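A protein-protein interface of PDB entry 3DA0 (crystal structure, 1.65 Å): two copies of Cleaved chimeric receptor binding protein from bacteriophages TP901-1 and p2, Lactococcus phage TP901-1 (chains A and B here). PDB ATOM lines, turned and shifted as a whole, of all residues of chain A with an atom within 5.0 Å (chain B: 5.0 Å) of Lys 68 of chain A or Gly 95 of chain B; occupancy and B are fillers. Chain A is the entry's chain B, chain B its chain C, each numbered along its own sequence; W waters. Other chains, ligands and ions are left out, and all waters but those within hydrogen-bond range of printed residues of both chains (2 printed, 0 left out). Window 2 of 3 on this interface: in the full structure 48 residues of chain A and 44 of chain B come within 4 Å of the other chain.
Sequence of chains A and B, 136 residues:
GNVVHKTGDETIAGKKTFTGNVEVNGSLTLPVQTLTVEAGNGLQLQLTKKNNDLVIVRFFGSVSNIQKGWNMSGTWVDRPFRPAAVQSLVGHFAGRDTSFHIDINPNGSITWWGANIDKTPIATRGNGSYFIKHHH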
ATOM      1  N   ILE A  66     -16.377  24.253   1.453  1.00  0.00           N
ATOM      2  CA  ILE A  66     -17.670  24.058   2.093  1.00  0.00           C
ATOM      3  C   ILE A  66     -18.445  23.148   1.193  1.00  0.00           C
ATOM      4  O   ILE A  66     -18.318  23.250  -0.020  1.00  0.00           O
ATOM      5  CB  ILE A  66     -18.379  25.418   2.327  1.00  0.00           C
ATOM      6  CG1 ILE A  66     -19.688  25.252   3.087  1.00  0.00           C
ATOM      7  CG2 ILE A  66     -18.612  26.198   1.032  1.00  0.00           C
ATOM      8  CD1 ILE A  66     -19.521  24.966   4.529  1.00  0.00           C
ATOM      9  N   GLN A  67     -19.201  22.232   1.776  1.00  0.00           N
ATOM     10  CA  GLN A  67     -20.081  21.417   0.980  1.00  0.00           C
ATOM     11  C   GLN A  67     -21.504  21.878   1.147  1.00  0.00           C
ATOM     12  O   GLN A  67     -21.880  22.412   2.182  1.00  0.00           O
ATOM     13  CB  GLN A  67     -19.979  19.929   1.343  1.00  0.00           C
ATOM     14  CG  GLN A  67     -18.576  19.369   1.241  1.00  0.00           C
ATOM     15  CD  GLN A  67     -18.539  17.847   1.348  1.00  0.00           C
ATOM     16  OE1 GLN A  67     -19.578  17.172   1.330  1.00  0.00           O
ATOM     17  NE2 GLN A  67     -17.344  17.300   1.455  1.00  0.00           N
ATOM     18  N   LYS A  68     -22.305  21.552   0.146  1.00  0.00           N
ATOM     19  CA  LYS A  68     -23.719  21.781   0.204  1.00  0.00           C
ATOM     20  C   LYS A  68     -24.338  21.058   1.373  1.00  0.00           C
ATOM     21  O   LYS A  68     -24.027  19.891   1.662  1.00  0.00           O
ATOM     22  CB  LYS A  68     -24.400  21.341  -1.104  1.00  0.00           C
ATOM     23  CG  LYS A  68     -24.489  19.843  -1.252  1.00  0.00           C
ATOM     24  CD  LYS A  68     -25.056  19.448  -2.589  1.00  0.00           C
ATOM     25  CE  LYS A  68     -24.064  19.769  -3.649  1.00  0.00           C
ATOM     26  NZ  LYS A  68     -24.611  19.559  -5.014  1.00  0.00           N
ATOM     27  N   GLY A  69     -25.201  21.799   2.065  1.00  0.00           N
ATOM     28  CA  GLY A  69     -25.936  21.312   3.201  1.00  0.00           C
ATOM     29  C   GLY A  69     -25.186  21.365   4.508  1.00  0.00           C
ATOM     30  O   GLY A  69     -25.750  21.059   5.532  1.00  0.00           O
ATOM     31  N   TRP A  70     -23.920  21.778   4.472  1.00  0.00           N
ATOM     32  CA  TRP A  70     -23.136  21.934   5.702  1.00  0.00           C
ATOM     33  C   TRP A  70     -23.395  23.260   6.345  1.00  0.00           C
ATOM     34  O   TRP A  70     -23.528  24.286   5.672  1.00  0.00           O
ATOM     35  CB  TRP A  70     -21.646  21.852   5.426  1.00  0.00           C
ATOM     36  CG  TRP A  70     -21.149  20.490   5.235  1.00  0.00           C
ATOM     37  CD1 TRP A  70     -21.883  19.356   5.083  1.00  0.00           C
ATOM     38  CD2 TRP A  70     -19.775  20.116   5.131  1.00  0.00           C
ATOM     39  NE1 TRP A  70     -21.039  18.266   4.927  1.00  0.00           N
ATOM     40  CE2 TRP A  70     -19.739  18.712   4.944  1.00  0.00           C
ATOM     41  CE3 TRP A  70     -18.570  20.834   5.187  1.00  0.00           C
ATOM     42  CZ2 TRP A  70     -18.551  18.011   4.801  1.00  0.00           C
ATOM     43  CZ3 TRP A  70     -17.381  20.133   5.071  1.00  0.00           C
ATOM     44  CH2 TRP A  70     -17.378  18.733   4.881  1.00  0.00           C
ATOM     45  N   TRP A 112     -24.871  26.271   4.100  1.00  0.00           N
ATOM     46  CA  TRP A 112     -24.459  26.573   2.720  1.00  0.00           C
ATOM     47  C   TRP A 112     -25.269  25.757   1.743  1.00  0.00           C
ATOM     48  O   TRP A 112     -25.378  24.517   1.868  1.00  0.00           O
ATOM     49  CB  TRP A 112     -22.968  26.252   2.557  1.00  0.00           C
ATOM     50  CG  TRP A 112     -22.524  26.449   1.211  1.00  0.00           C
ATOM     51  CD1 TRP A 112     -22.244  25.474   0.299  1.00  0.00           C
ATOM     52  CD2 TRP A 112     -22.207  27.689   0.599  1.00  0.00           C
ATOM     53  NE1 TRP A 112     -21.846  26.043  -0.869  1.00  0.00           N
ATOM     54  CE2 TRP A 112     -21.776  27.403  -0.705  1.00  0.00           C
ATOM     55  CE3 TRP A 112     -22.247  29.019   1.021  1.00  0.00           C
ATOM     56  CZ2 TRP A 112     -21.438  28.404  -1.604  1.00  0.00           C
ATOM     57  CZ3 TRP A 112     -21.906  30.012   0.160  1.00  0.00           C
ATOM     58  CH2 TRP A 112     -21.499  29.699  -1.165  1.00  0.00           C
ATOM     59  N   TRP A 113     -25.825  26.421   0.723  1.00  0.00           N
ATOM     60  CA  TRP A 113     -26.529  25.701  -0.293  1.00  0.00           C
ATOM     61  C   TRP A 113     -26.105  26.071  -1.687  1.00  0.00           C
ATOM     62  O   TRP A 113     -26.871  25.862  -2.638  1.00  0.00           O
ATOM     63  CB  TRP A 113     -28.047  25.832  -0.146  1.00  0.00           C
ATOM     64  CG  TRP A 113     -28.564  24.966   0.954  1.00  0.00           C
ATOM     65  CD1 TRP A 113     -29.020  25.364   2.159  1.00  0.00           C
ATOM     66  CD2 TRP A 113     -28.662  23.534   0.931  1.00  0.00           C
ATOM     67  NE1 TRP A 113     -29.382  24.267   2.915  1.00  0.00           N
ATOM     68  CE2 TRP A 113     -29.202  23.137   2.171  1.00  0.00           C
ATOM     69  CE3 TRP A 113     -28.384  22.556  -0.038  1.00  0.00           C
ATOM     70  CZ2 TRP A 113     -29.437  21.800   2.486  1.00  0.00           C
ATOM     71  CZ3 TRP A 113     -28.627  21.215   0.273  1.00  0.00           C
ATOM     72  CH2 TRP A 113     -29.153  20.865   1.528  1.00  0.00           C
ATOM     73  N   GLY A 114     -24.882  26.548  -1.868  1.00  0.00           N
ATOM     74  CA  GLY A 114     -24.303  26.491  -3.200  1.00  0.00           C
ATOM     75  C   GLY A 114     -23.809  25.098  -3.493  1.00  0.00           C
ATOM     76  O   GLY A 114     -24.045  24.136  -2.735  1.00  0.00           O
ATOM     77  N   ALA A 115     -23.141  24.983  -4.634  1.00  0.00           N
ATOM     78  CA  ALA A 115     -22.376  23.789  -4.924  1.00  0.00           C
ATOM     79  C   ALA A 115     -21.249  23.595  -3.943  1.00  0.00           C
ATOM     80  O   ALA A 115     -20.874  24.506  -3.220  1.00  0.00           O
ATOM     81  CB  ALA A 115     -21.860  23.838  -6.408  1.00  0.00           C
ATOM     82  N   ASN A 116     -20.665  22.390  -3.905  1.00  0.00           N
ATOM     83  CA  ASN A 116     -19.452  22.235  -3.137  1.00  0.00           C
ATOM     84  C   ASN A 116     -18.348  23.147  -3.681  1.00  0.00           C
ATOM     85  O   ASN A 116     -18.126  23.253  -4.903  1.00  0.00           O
ATOM     86  CB  ASN A 116     -18.985  20.780  -3.133  1.00  0.00           C
ATOM     87  CG  ASN A 116     -19.961  19.843  -2.463  1.00  0.00           C
ATOM     88  OD1 ASN A 116     -20.900  20.263  -1.803  1.00  0.00           O
ATOM     89  ND2 ASN A 116     -19.743  18.529  -2.653  1.00  0.00           N
ATOM     90  N   HIS B  92     -32.760  30.247  -6.685  1.00  0.00           N
ATOM     91  CA  HIS B  92     -31.508  29.498  -6.788  1.00  0.00           C
ATOM     92  C   HIS B  92     -31.815  28.018  -6.686  1.00  0.00           C
ATOM     93  O   HIS B  92     -32.709  27.617  -6.008  1.00  0.00           O
ATOM     94  CB  HIS B  92     -30.550  29.913  -5.690  1.00  0.00           C
ATOM     95  CG  HIS B  92     -29.267  29.171  -5.731  1.00  0.00           C
ATOM     96  ND1 HIS B  92     -28.920  28.278  -4.757  1.00  0.00           N
ATOM     97  CD2 HIS B  92     -28.279  29.129  -6.655  1.00  0.00           C
ATOM     98  CE1 HIS B  92     -27.759  27.721  -5.063  1.00  0.00           C
ATOM     99  NE2 HIS B  92     -27.355  28.214  -6.221  1.00  0.00           N
ATOM    100  N   PHE B  93     -31.081  27.202  -7.434  1.00  0.00           N
ATOM    101  CA  PHE B  93     -31.259  25.766  -7.333  1.00  0.00           C
ATOM    102  C   PHE B  93     -30.355  25.189  -6.206  1.00  0.00           C
ATOM    103  O   PHE B  93     -29.124  25.325  -6.277  1.00  0.00           O
ATOM    104  CB  PHE B  93     -30.900  25.106  -8.682  1.00  0.00           C
ATOM    105  CG  PHE B  93     -31.873  25.405  -9.745  1.00  0.00           C
ATOM    106  CD1 PHE B  93     -33.163  24.944  -9.631  1.00  0.00           C
ATOM    107  CD2 PHE B  93     -31.482  26.055 -10.929  1.00  0.00           C
ATOM    108  CE1 PHE B  93     -34.085  25.216 -10.622  1.00  0.00           C
ATOM    109  CE2 PHE B  93     -32.425  26.334 -11.920  1.00  0.00           C
ATOM    110  CZ  PHE B  93     -33.701  25.895 -11.755  1.00  0.00           C
ATOM    111  N   ALA B  94     -30.968  24.585  -5.194  1.00  0.00           N
ATOM    112  CA  ALA B  94     -30.254  24.152  -3.994  1.00  0.00           C
ATOM    113  C   ALA B  94     -29.098  23.227  -4.363  1.00  0.00           C
ATOM    114  O   ALA B  94     -29.290  22.228  -5.036  1.00  0.00           O
ATOM    115  CB  ALA B  94     -31.218  23.442  -2.997  1.00  0.00           C
ATOM    116  N   GLY B  95     -27.910  23.535  -3.838  1.00  0.00           N
ATOM    117  CA  GLY B  95     -26.759  22.692  -4.022  1.00  0.00           C
ATOM    118  C   GLY B  95     -26.083  22.829  -5.378  1.00  0.00           C
ATOM    119  O   GLY B  95     -25.224  21.989  -5.734  1.00  0.00           O
ATOM    120  N   ARG B  96     -26.487  23.839  -6.162  1.00  0.00           N
ATOM    121  CA  ARG B  96     -25.993  24.072  -7.516  1.00  0.00           C
ATOM    122  C   ARG B  96     -25.471  25.468  -7.707  1.00  0.00           C
ATOM    123  O   ARG B  96     -25.691  26.299  -6.874  1.00  0.00           O
ATOM    124  CB  ARG B  96     -27.080  23.827  -8.512  1.00  0.00           C
ATOM    125  CG  ARG B  96     -27.759  22.481  -8.283  1.00  0.00           C
ATOM    126  CD  ARG B  96     -28.505  22.041  -9.428  1.00  0.00           C
ATOM    127  NE  ARG B  96     -29.019  20.709  -9.152  1.00  0.00           N
ATOM    128  CZ  ARG B  96     -29.300  19.808 -10.075  1.00  0.00           C
ATOM    129  NH1 ARG B  96     -29.797  18.644  -9.687  1.00  0.00           N
ATOM    130  NH2 ARG B  96     -29.105  20.064 -11.369  1.00  0.00           N
ATOM    131  N   ASP B  97     -24.803  25.689  -8.845  1.00  0.00           N
ATOM    132  CA  ASP B  97     -24.310  27.013  -9.265  1.00  0.00           C
ATOM    133  C   ASP B  97     -25.325  27.790 -10.077  1.00  0.00           C
ATOM    134  O   ASP B  97     -25.071  28.919 -10.490  1.00  0.00           O
ATOM    135  CB  ASP B  97     -23.131  26.880 -10.178  1.00  0.00           C
ATOM    136  CG  ASP B  97     -21.901  26.492  -9.479  1.00  0.00           C
ATOM    137  OD1 ASP B  97     -21.736  26.873  -8.294  1.00  0.00           O
ATOM    138  OD2 ASP B  97     -21.075  25.802 -10.140  1.00  0.00           O
HETATM  139  O   HOH W   1     -23.751  20.393  -7.102  1.00  0.00           O
HETATM  140  O   HOH W   2     -22.870  27.449  -5.938  1.00  0.00           O
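No position is printed for both chains.
Water W1 lies within hydrogen-bond range of the side-chain amino group of Lys 68 of chain A and the backbone carbonyl oxygen of Gly 95 of chain B. Water W2 lies within hydrogen-bond range of OD1 of Asp 97 of chain B (2.7 Å), N of Ala 115 of chain A (2.8 Å) and O of Arg 96 of chain B (3.2 Å).
Lys 68 of chain A touches one residue of chain B. Trp 112 of chain A touches none of the printed residues of chain B. Of the printed residues of chain B, Gly 114 of chain A touches Gly 95 (3.3 Å) and Arg 96 (3.9 Å). Printed residues of chain A within 4 Å of His 92 of chain B: Trp 113. Phe 93 of chain B touches none of the printed residues of chain A. Of the printed residues of chain A, Ala 94 of chain B touches Trp 113. Gly 95 of chain B touches just these residues of chain A: Lys 68 (2.6 Å), Trp 113 (2.8 Å), Gly 114 (3.3 Å) and Ala 115 (3.5 Å). Of the printed residues of chain A, Arg 96 of chain B touches Gly 114 and Ala 115. Printed residues of chain A within 4 Å of Asp 97 of chain B: Ala 115. The nearest residue of chain B that does not touch Lys 68 of chain A is Arg 96 of chain B (4.8 Å). The nearest printed residue of chain A that does not touch Ala 94 of chain B is Gly 114 of chain A (5.4 Å).
The side-chain amino group of Lys 68 of chain A is in hydrogen-bond range of the backbone carbonyl oxygen of Gly 95 of chain B, at 2.6 Å. The backbone NH (N) of Gly 95 of chain B lies within hydrogen-bond range of the backbone carbonyl oxygen (O) of Trp 113 of chain A (2.8 Å).
OD1 of Asn 116 of chain A lies within hydrogen-bond range of N of Lys 68 of chain A, 2.7 Å away. O of Gly 114 of chain A sits close to NE1 of Trp 112 of chain A, 3.5 Å away. The backbone carbonyl oxygen (O) of Ala 115 of chain A sits at hydrogen-bond distance from the indole nitrogen (NE1) of Trp 112 of chain A. NE2 of His 92 of chain B lies within hydrogen-bond range of O of Arg 96 of chain B (2.6 Å).
Among the printed residues, pairs that only touch across the chains: Trp 113 of chain A with His 92 of chain B (3.2 Å), Gly 114 of chain A with Gly 95 of chain B (3.3 Å), Ala 115 of chain A with Gly 95 of chain B (3.5 Å), Ala 115 of chain A with Asp 97 of chain B (3.6 Å), Ala 115 of chain A with Arg 96 of chain B (3.6 Å), Trp 113 of chain A with Ala 94 of chain B (3.9 Å) and Gly 114 of chain A with Arg 96 of chain B (3.9 Å).
Hydrophobic or aromatic side chains of chain B within 4 Å of the printed part of chain A: His 92. Of the 10 printed residues of chain A, 4 touch a printed residue of chain B. Hydrophobic or aromatic side chains of chain A that line the printed part of chain B: Trp 113 and Ala 115. Along chain A the printed residues that touch a printed residue of chain B span positions 68 to 115. Among the printed residues, no Asp or Glu carboxylate lies within 4 Å of a Lys or Arg side-chain nitrogen of the other chain.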
